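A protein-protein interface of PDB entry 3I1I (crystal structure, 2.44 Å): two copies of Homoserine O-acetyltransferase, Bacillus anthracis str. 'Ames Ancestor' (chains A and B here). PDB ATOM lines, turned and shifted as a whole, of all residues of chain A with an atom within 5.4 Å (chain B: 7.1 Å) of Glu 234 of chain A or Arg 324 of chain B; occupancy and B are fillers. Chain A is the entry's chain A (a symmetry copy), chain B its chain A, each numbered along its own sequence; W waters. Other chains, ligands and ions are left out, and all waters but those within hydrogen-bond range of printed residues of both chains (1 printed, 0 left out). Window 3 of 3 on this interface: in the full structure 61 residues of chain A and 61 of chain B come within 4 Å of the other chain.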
ATOM      1  N   PHE A 232       1.483 -19.841   8.577  1.00  0.00           N
ATOM      2  CA  PHE A 232       0.440 -19.634   7.543  1.00  0.00           C
ATOM      3  C   PHE A 232       0.517 -18.178   7.037  1.00  0.00           C
ATOM      4  O   PHE A 232       1.333 -17.411   7.531  1.00  0.00           O
ATOM      5  CB  PHE A 232      -0.953 -19.920   8.103  1.00  0.00           C
ATOM      6  CG  PHE A 232      -1.157 -21.338   8.633  1.00  0.00           C
ATOM      7  CD1 PHE A 232      -1.709 -22.323   7.834  1.00  0.00           C
ATOM      8  CD2 PHE A 232      -0.832 -21.657   9.937  1.00  0.00           C
ATOM      9  CE1 PHE A 232      -1.899 -23.652   8.316  1.00  0.00           C
ATOM     10  CE2 PHE A 232      -1.008 -22.966  10.445  1.00  0.00           C
ATOM     11  CZ  PHE A 232      -1.542 -23.974   9.625  1.00  0.00           C
ATOM     12  N   ASP A 233      -0.292 -17.804   6.057  1.00  0.00           N
ATOM     13  CA  ASP A 233      -0.455 -16.391   5.657  1.00  0.00           C
ATOM     14  C   ASP A 233      -1.201 -15.667   6.759  1.00  0.00           C
ATOM     15  O   ASP A 233      -1.964 -16.284   7.493  1.00  0.00           O
ATOM     16  CB  ASP A 233      -1.313 -16.301   4.395  1.00  0.00           C
ATOM     17  CG  ASP A 233      -1.444 -14.882   3.852  1.00  0.00           C
ATOM     18  OD1 ASP A 233      -0.504 -14.391   3.171  1.00  0.00           O
ATOM     19  OD2 ASP A 233      -2.514 -14.261   4.072  1.00  0.00           O
ATOM     20  N   GLU A 234      -1.001 -14.349   6.883  1.00  0.00           N
ATOM     21  CA  GLU A 234      -1.696 -13.607   7.920  1.00  0.00           C
ATOM     22  C   GLU A 234      -3.232 -13.733   7.833  1.00  0.00           C
ATOM     23  O   GLU A 234      -3.931 -13.818   8.848  1.00  0.00           O
ATOM     24  CB  GLU A 234      -1.260 -12.143   7.932  1.00  0.00           C
ATOM     25  CG  GLU A 234      -1.649 -11.315   6.739  1.00  0.00           C
ATOM     26  CD  GLU A 234      -3.066 -10.794   6.805  1.00  0.00           C
ATOM     27  OE1 GLU A 234      -3.478 -10.205   5.790  1.00  0.00           O
ATOM     28  OE2 GLU A 234      -3.760 -10.978   7.837  1.00  0.00           O
ATOM     29  N   HIS A 235      -3.739 -13.757   6.627  1.00  0.00           N
ATOM     30  CA  HIS A 235      -5.148 -13.818   6.446  1.00  0.00           C
ATOM     31  C   HIS A 235      -5.748 -15.157   6.896  1.00  0.00           C
ATOM     32  O   HIS A 235      -6.920 -15.230   7.260  1.00  0.00           O
ATOM     33  CB  HIS A 235      -5.512 -13.535   5.001  1.00  0.00           C
ATOM     34  CG  HIS A 235      -6.938 -13.131   4.841  1.00  0.00           C
ATOM     35  ND1 HIS A 235      -7.821 -13.804   4.025  1.00  0.00           N
ATOM     36  CD2 HIS A 235      -7.648 -12.148   5.442  1.00  0.00           C
ATOM     37  CE1 HIS A 235      -9.007 -13.229   4.108  1.00  0.00           C
ATOM     38  NE2 HIS A 235      -8.927 -12.219   4.956  1.00  0.00           N
ATOM     39  N   PHE A 236      -4.943 -16.205   6.886  1.00  0.00           N
ATOM     40  CA  PHE A 236      -5.385 -17.466   7.430  1.00  0.00           C
ATOM     41  C   PHE A 236      -5.831 -17.297   8.871  1.00  0.00           C
ATOM     42  O   PHE A 236      -6.868 -17.836   9.230  1.00  0.00           O
ATOM     43  CB  PHE A 236      -4.303 -18.540   7.346  1.00  0.00           C
ATOM     44  CG  PHE A 236      -4.686 -19.840   8.003  1.00  0.00           C
ATOM     45  CD1 PHE A 236      -5.374 -20.805   7.303  1.00  0.00           C
ATOM     46  CD2 PHE A 236      -4.371 -20.070   9.339  1.00  0.00           C
ATOM     47  CE1 PHE A 236      -5.731 -22.026   7.910  1.00  0.00           C
ATOM     48  CE2 PHE A 236      -4.721 -21.258   9.963  1.00  0.00           C
ATOM     49  CZ  PHE A 236      -5.400 -22.266   9.245  1.00  0.00           C
ATOM     50  N   TYR A 237      -5.062 -16.585   9.695  1.00  0.00           N
ATOM     51  CA  TYR A 237      -5.422 -16.466  11.130  1.00  0.00           C
ATOM     52  C   TYR A 237      -6.657 -15.564  11.332  1.00  0.00           C
ATOM     53  O   TYR A 237      -7.457 -15.777  12.251  1.00  0.00           O
ATOM     54  CB  TYR A 237      -4.255 -15.923  11.956  1.00  0.00           C
ATOM     55  CG  TYR A 237      -2.953 -16.675  11.748  1.00  0.00           C
ATOM     56  CD1 TYR A 237      -2.671 -17.817  12.471  1.00  0.00           C
ATOM     57  CD2 TYR A 237      -2.011 -16.240  10.822  1.00  0.00           C
ATOM     58  CE1 TYR A 237      -1.489 -18.502  12.285  1.00  0.00           C
ATOM     59  CE2 TYR A 237      -0.843 -16.921  10.618  1.00  0.00           C
ATOM     60  CZ  TYR A 237      -0.582 -18.057  11.351  1.00  0.00           C
ATOM     61  OH  TYR A 237       0.580 -18.736  11.187  1.00  0.00           O
ATOM     62  N   GLU A 238      -6.780 -14.559  10.467  1.00  0.00           N
ATOM     63  CA  GLU A 238      -7.849 -13.591  10.522  1.00  0.00           C
ATOM     64  C   GLU A 238      -9.207 -14.255  10.259  1.00  0.00           C
ATOM     65  O   GLU A 238     -10.185 -13.951  10.964  1.00  0.00           O
ATOM     66  CB  GLU A 238      -7.602 -12.462   9.507  1.00  0.00           C
ATOM     67  CG  GLU A 238      -8.345 -11.204   9.798  1.00  0.00           C
ATOM     68  CD  GLU A 238      -7.839 -10.436  11.065  1.00  0.00           C
ATOM     69  OE1 GLU A 238      -6.651 -10.562  11.453  1.00  0.00           O
ATOM     70  OE2 GLU A 238      -8.669  -9.699  11.682  1.00  0.00           O
ATOM     71  N   LEU A 319       5.974 -16.787   5.400  1.00  0.00           N
ATOM     72  CA  LEU A 319       6.592 -15.825   6.285  1.00  0.00           C
ATOM     73  C   LEU A 319       7.856 -16.346   6.954  1.00  0.00           C
ATOM     74  O   LEU A 319       8.668 -15.544   7.502  1.00  0.00           O
ATOM     75  CB  LEU A 319       5.632 -15.404   7.378  1.00  0.00           C
ATOM     76  CG  LEU A 319       4.330 -14.693   6.984  1.00  0.00           C
ATOM     77  CD1 LEU A 319       3.353 -14.763   8.188  1.00  0.00           C
ATOM     78  CD2 LEU A 319       4.533 -13.241   6.524  1.00  0.00           C
ATOM     79  N   ASN B 181      -4.736  -0.084  11.483  1.00  0.00           N
ATOM     80  CA  ASN B 181      -5.888  -0.893  11.009  1.00  0.00           C
ATOM     81  C   ASN B 181      -7.058  -0.694  11.970  1.00  0.00           C
ATOM     82  O   ASN B 181      -6.846  -0.323  13.143  1.00  0.00           O
ATOM     83  CB  ASN B 181      -5.540  -2.378  10.956  1.00  0.00           C
ATOM     84  CG  ASN B 181      -4.975  -2.792   9.635  1.00  0.00           C
ATOM     85  OD1 ASN B 181      -5.516  -2.425   8.600  1.00  0.00           O
ATOM     86  ND2 ASN B 181      -3.871  -3.541   9.648  1.00  0.00           N
ATOM     87  N   PRO B 185      -4.833  -6.949  13.781  1.00  0.00           N
ATOM     88  CA  PRO B 185      -4.835  -8.273  13.174  1.00  0.00           C
ATOM     89  C   PRO B 185      -4.569  -9.364  14.182  1.00  0.00           C
ATOM     90  O   PRO B 185      -3.849  -9.152  15.157  1.00  0.00           O
ATOM     91  CB  PRO B 185      -3.705  -8.203  12.159  1.00  0.00           C
ATOM     92  CG  PRO B 185      -3.636  -6.748  11.808  1.00  0.00           C
ATOM     93  CD  PRO B 185      -3.897  -6.032  13.122  1.00  0.00           C
ATOM     94  N   ILE B 186      -5.184 -10.508  13.951  1.00  0.00           N
ATOM     95  CA  ILE B 186      -5.049 -11.659  14.834  1.00  0.00           C
ATOM     96  C   ILE B 186      -3.572 -12.071  14.955  1.00  0.00           C
ATOM     97  O   ILE B 186      -3.103 -12.323  16.050  1.00  0.00           O
ATOM     98  CB  ILE B 186      -5.874 -12.870  14.296  1.00  0.00           C
ATOM     99  CG1 ILE B 186      -7.362 -12.519  14.242  1.00  0.00           C
ATOM    100  CG2 ILE B 186      -5.645 -14.129  15.151  1.00  0.00           C
ATOM    101  CD1 ILE B 186      -7.976 -12.071  15.592  1.00  0.00           C
ATOM    102  N   ILE B 187      -2.854 -12.105  13.830  1.00  0.00           N
ATOM    103  CA  ILE B 187      -1.439 -12.504  13.825  1.00  0.00           C
ATOM    104  C   ILE B 187      -0.619 -11.631  14.738  1.00  0.00           C
ATOM    105  O   ILE B 187       0.177 -12.144  15.540  1.00  0.00           O
ATOM    106  CB  ILE B 187      -0.825 -12.514  12.409  1.00  0.00           C
ATOM    107  CG1 ILE B 187       0.556 -13.174  12.405  1.00  0.00           C
ATOM    108  CG2 ILE B 187      -0.747 -11.078  11.754  1.00  0.00           C
ATOM    109  CD1 ILE B 187       1.060 -13.494  10.868  1.00  0.00           C
ATOM    110  N   THR B 188      -0.823 -10.320  14.654  1.00  0.00           N
ATOM    111  CA  THR B 188      -0.129  -9.397  15.525  1.00  0.00           C
ATOM    112  C   THR B 188      -0.626  -9.482  16.985  1.00  0.00           C
ATOM    113  O   THR B 188       0.137  -9.369  17.930  1.00  0.00           O
ATOM    114  CB  THR B 188      -0.309  -7.969  14.995  1.00  0.00           C
ATOM    115  OG1 THR B 188       0.068  -7.931  13.622  1.00  0.00           O
ATOM    116  CG2 THR B 188       0.492  -6.962  15.797  1.00  0.00           C
ATOM    117  N   PRO B 314      -1.054   3.025   4.719  1.00  0.00           N
ATOM    118  CA  PRO B 314      -0.343   1.817   5.098  1.00  0.00           C
ATOM    119  C   PRO B 314       0.972   1.664   4.303  1.00  0.00           C
ATOM    120  O   PRO B 314       1.182   2.316   3.278  1.00  0.00           O
ATOM    121  CB  PRO B 314      -1.312   0.724   4.692  1.00  0.00           C
ATOM    122  CG  PRO B 314      -1.932   1.235   3.487  1.00  0.00           C
ATOM    123  CD  PRO B 314      -2.093   2.723   3.719  1.00  0.00           C
ATOM    124  N   LEU B 319       4.547  -5.844   8.284  1.00  0.00           N
ATOM    125  CA  LEU B 319       4.196  -7.144   8.812  1.00  0.00           C
ATOM    126  C   LEU B 319       3.289  -7.074  10.033  1.00  0.00           C
ATOM    127  O   LEU B 319       2.654  -8.100  10.418  1.00  0.00           O
ATOM    128  CB  LEU B 319       5.437  -7.920   9.203  1.00  0.00           C
ATOM    129  CG  LEU B 319       6.459  -8.276   8.114  1.00  0.00           C
ATOM    130  CD1 LEU B 319       7.794  -8.659   8.807  1.00  0.00           C
ATOM    131  CD2 LEU B 319       5.989  -9.393   7.168  1.00  0.00           C
ATOM    132  N   GLN B 321       0.906  -4.579  10.527  1.00  0.00           N
ATOM    133  CA  GLN B 321      -0.371  -4.042  10.129  1.00  0.00           C
ATOM    134  C   GLN B 321      -0.575  -4.233   8.624  1.00  0.00           C
ATOM    135  O   GLN B 321      -0.331  -3.316   7.825  1.00  0.00           O
ATOM    136  CB  GLN B 321      -0.439  -2.553  10.501  1.00  0.00           C
ATOM    137  CG  GLN B 321      -0.455  -2.261  12.033  1.00  0.00           C
ATOM    138  CD  GLN B 321      -1.610  -2.932  12.751  1.00  0.00           C
ATOM    139  OE1 GLN B 321      -2.637  -3.296  12.144  1.00  0.00           O
ATOM    140  NE2 GLN B 321      -1.431  -3.160  14.023  1.00  0.00           N
ATOM    141  N   PRO B 322      -1.020  -5.437   8.226  1.00  0.00           N
ATOM    142  CA  PRO B 322      -1.189  -5.740   6.815  1.00  0.00           C
ATOM    143  C   PRO B 322      -2.128  -4.762   6.140  1.00  0.00           C
ATOM    144  O   PRO B 322      -3.201  -4.441   6.653  1.00  0.00           O
ATOM    145  CB  PRO B 322      -1.790  -7.129   6.848  1.00  0.00           C
ATOM    146  CG  PRO B 322      -1.275  -7.723   8.108  1.00  0.00           C
ATOM    147  CD  PRO B 322      -1.305  -6.606   9.068  1.00  0.00           C
ATOM    148  N   SER B 323      -1.741  -4.274   4.994  1.00  0.00           N
ATOM    149  CA  SER B 323      -2.475  -3.191   4.408  1.00  0.00           C
ATOM    150  C   SER B 323      -3.839  -3.621   3.835  1.00  0.00           C
ATOM    151  O   SER B 323      -4.720  -2.780   3.601  1.00  0.00           O
ATOM    152  CB  SER B 323      -1.623  -2.536   3.331  1.00  0.00           C
ATOM    153  OG  SER B 323      -1.585  -3.368   2.220  1.00  0.00           O
ATOM    154  N   ARG B 324      -4.058  -4.913   3.599  1.00  0.00           N
ATOM    155  CA  ARG B 324      -5.345  -5.274   2.985  1.00  0.00           C
ATOM    156  C   ARG B 324      -6.565  -4.761   3.791  1.00  0.00           C
ATOM    157  O   ARG B 324      -7.586  -4.465   3.218  1.00  0.00           O
ATOM    158  CB  ARG B 324      -5.483  -6.773   2.730  1.00  0.00           C
ATOM    159  CG  ARG B 324      -5.573  -7.558   3.995  1.00  0.00           C
ATOM    160  CD  ARG B 324      -5.528  -9.043   3.723  1.00  0.00           C
ATOM    161  NE  ARG B 324      -6.720  -9.496   3.036  1.00  0.00           N
ATOM    162  CZ  ARG B 324      -6.801 -10.573   2.256  1.00  0.00           C
ATOM    163  NH1 ARG B 324      -5.768 -11.355   2.035  1.00  0.00           N
ATOM    164  NH2 ARG B 324      -7.951 -10.882   1.723  1.00  0.00           N
ATOM    165  N   TYR B 325      -6.460  -4.657   5.105  1.00  0.00           N
ATOM    166  CA  TYR B 325      -7.616  -4.228   5.892  1.00  0.00           C
ATOM    167  C   TYR B 325      -7.825  -2.724   5.795  1.00  0.00           C
ATOM    168  O   TYR B 325      -8.918  -2.260   6.066  1.00  0.00           O
ATOM    169  CB  TYR B 325      -7.497  -4.688   7.344  1.00  0.00           C
ATOM    170  CG  TYR B 325      -7.176  -6.156   7.432  1.00  0.00           C
ATOM    171  CD1 TYR B 325      -8.113  -7.106   7.055  1.00  0.00           C
ATOM    172  CD2 TYR B 325      -5.905  -6.587   7.813  1.00  0.00           C
ATOM    173  CE1 TYR B 325      -7.811  -8.468   7.080  1.00  0.00           C
ATOM    174  CE2 TYR B 325      -5.590  -7.941   7.872  1.00  0.00           C
ATOM    175  CZ  TYR B 325      -6.534  -8.881   7.496  1.00  0.00           C
ATOM    176  OH  TYR B 325      -6.217 -10.219   7.530  1.00  0.00           O
ATOM    177  N   ASN B 326      -6.812  -1.950   5.379  1.00  0.00           N
ATOM    178  CA  ASN B 326      -7.064  -0.529   5.086  1.00  0.00           C
ATOM    179  C   ASN B 326      -7.988  -0.417   3.856  1.00  0.00           C
ATOM    180  O   ASN B 326      -8.930   0.414   3.822  1.00  0.00           O
ATOM    181  CB  ASN B 326      -5.780   0.247   4.831  1.00  0.00           C
ATOM    182  CG  ASN B 326      -4.986   0.585   6.087  1.00  0.00           C
ATOM    183  OD1 ASN B 326      -4.236   1.557   6.063  1.00  0.00           O
ATOM    184  ND2 ASN B 326      -5.135  -0.180   7.161  1.00  0.00           N
ATOM    185  N   TYR B 327      -7.727  -1.251   2.843  1.00  0.00           N
ATOM    186  CA  TYR B 327      -8.542  -1.248   1.615  1.00  0.00           C
ATOM    187  C   TYR B 327      -9.965  -1.657   1.904  1.00  0.00           C
ATOM    188  O   TYR B 327     -10.917  -1.055   1.398  1.00  0.00           O
ATOM    189  CB  TYR B 327      -7.943  -2.153   0.553  1.00  0.00           C
ATOM    190  CG  TYR B 327      -6.696  -1.573  -0.063  1.00  0.00           C
ATOM    191  CD1 TYR B 327      -6.769  -0.597  -1.061  1.00  0.00           C
ATOM    192  CD2 TYR B 327      -5.440  -1.951   0.392  1.00  0.00           C
ATOM    193  CE1 TYR B 327      -5.611  -0.012  -1.599  1.00  0.00           C
ATOM    194  CE2 TYR B 327      -4.280  -1.400  -0.142  1.00  0.00           C
ATOM    195  CZ  TYR B 327      -4.370  -0.443  -1.140  1.00  0.00           C
ATOM    196  OH  TYR B 327      -3.199   0.061  -1.659  1.00  0.00           O
ATOM    197  N   LYS B 328     -10.136  -2.661   2.757  1.00  0.00           N
ATOM    198  CA  LYS B 328     -11.483  -3.108   3.096  1.00  0.00           C
ATOM    199  C   LYS B 328     -12.274  -1.955   3.734  1.00  0.00           C
ATOM    200  O   LYS B 328     -13.378  -1.633   3.301  1.00  0.00           O
ATOM    201  CB  LYS B 328     -11.417  -4.312   4.037  1.00  0.00           C
ATOM    202  CG  LYS B 328     -12.754  -4.863   4.463  1.00  0.00           C
ATOM    203  CD  LYS B 328     -13.427  -5.679   3.335  1.00  0.00           C
ATOM    204  CE  LYS B 328     -14.614  -4.962   2.679  1.00  0.00           C
ATOM    205  NZ  LYS B 328     -15.787  -5.887   2.707  1.00  0.00           N
ATOM    206  N   MET B 329     -11.689  -1.333   4.742  1.00  0.00           N
ATOM    207  CA  MET B 329     -12.314  -0.237   5.487  1.00  0.00           C
ATOM    208  C   MET B 329     -12.695   0.931   4.586  1.00  0.00           C
ATOM    209  O   MET B 329     -13.797   1.474   4.681  1.00  0.00           O
ATOM    210  CB  MET B 329     -11.363   0.228   6.582  1.00  0.00           C
ATOM    211  CG  MET B 329     -11.604   1.627   7.093  1.00  0.00           C
ATOM    212  SD  MET B 329     -10.471   1.991   8.626  1.00  0.00           S
ATOM    213  CE  MET B 329     -10.920   3.873   8.970  1.00  0.00           C
ATOM    214  N   GLU B 344      -0.900   4.108  -0.256  1.00  0.00           N
ATOM    215  CA  GLU B 344       0.022   3.048   0.165  1.00  0.00           C
ATOM    216  C   GLU B 344       1.459   3.381  -0.173  1.00  0.00           C
ATOM    217  O   GLU B 344       1.786   3.672  -1.304  1.00  0.00           O
ATOM    218  CB  GLU B 344      -0.348   1.712  -0.481  1.00  0.00           C
ATOM    219  CG  GLU B 344       0.496   0.575   0.065  1.00  0.00           C
ATOM    220  CD  GLU B 344      -0.113  -0.795  -0.186  1.00  0.00           C
ATOM    221  OE1 GLU B 344      -0.593  -1.032  -1.303  1.00  0.00           O
ATOM    222  OE2 GLU B 344      -0.110  -1.649   0.718  1.00  0.00           O
HETATM  223  O   HOH W   1      -4.146 -12.055  11.215  1.00  0.00           O
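Hydrophobic or aromatic side chains of chain B that line the printed part of chain A: Pro 185, Ile 186, Ile 187, Pro 322 and Tyr 325.
Among the printed residues, 12 pairs touch across the chains.
Among the printed residues, no Asp or Glu carboxylate lies within 4 Å of a Lys or Arg side-chain nitrogen of the other chain.
The side-chain carboxylate (OE2) of Glu 234 of chain A lies within hydrogen-bond range of the side-chain hydroxyl (OH) of Tyr 325 of chain B (2.6 Å).
The backbone NH of Ile 186 of chain B lies within hydrogen-bond range of the side-chain carboxylate of Glu 238 of chain A (2.9 Å).
The backbone NH (N) of His 235 of chain A sits at hydrogen-bond distance from the side-chain carboxylate (OD2) of Asp 233 of chain A.
The side-chain amide nitrogen (ND2) of Asn 181 of chain B is in hydrogen-bond range of the backbone carbonyl oxygen (O) of Pro 322 of chain B, at 3.2 Å.
The side-chain hydroxyl (OH) of Tyr 237 of chain A sits at hydrogen-bond distance from the backbone NH (N) of Phe 232 of chain A, 3.0 Å away.
Among the printed residues, pairs that only touch across the chains: Glu 234 of chain A with Arg 324 of chain B (3.1 Å), His 235 of chain A with Tyr 325 of chain B (3.2 Å), Glu 238 of chain A with Tyr 325 of chain B (3.3 Å), Glu 238 of chain A with Pro 185 of chain B (3.4 Å), His 235 of chain A with Arg 324 of chain B (3.5 Å), Glu 234 of chain A with Pro 322 of chain B (3.7 Å), Leu 319 of chain A with Ile 187 of chain B (3.7 Å), Tyr 237 of chain A with Ile 186 of chain B (3.8 Å), Tyr 237 of chain A with Ile 187 of chain B (3.9 Å) and Glu 234 of chain A with Ile 187 of chain B (3.98 Å).
Glu 234 of chain A touches just these residues of chain B: Ile 187, Pro 322, Arg 324 and Tyr 325.
Of the printed residues of chain B, His 235 of chain A touches Arg 324 (3.5 Å) and Tyr 325 (3.2 Å).
Of the printed residues of chain B, Tyr 237 of chain A touches Ile 186 and Ile 187.
Of the printed residues of chain B, Leu 319 of chain A touches Ile 187.
Printed residues of chain A within 4 Å of Pro 185 of chain B: Glu 238 (3.4 Å).
Of the printed residues of chain A, Ile 186 of chain B touches Tyr 237 and Glu 238.
Arg 324 of chain B touches two residues of chain A.
Met 329 of chain B touches none of the printed residues of chain A.
The nearest residue of chain A that does not touch Arg 324 of chain B is Asp 233 of chain A (4.8 Å).
The nearest printed residue of chain A that does not touch Tyr 325 of chain B is Phe 236 of chain A (6.2 Å).
Water W1 lies within hydrogen-bond range of N of Ile 187 of chain B (2.9 Å), OE1 of Glu 238 of chain A (2.9 Å), O of Glu 234 of chain A (3.0 Å) and N of Ile 186 of chain B (3.3 Å).
Position printed for both chains: 319.
Of the 12 pairs that touch across the chains among the printed residues, none has its exchanged pair printed and touching as well.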
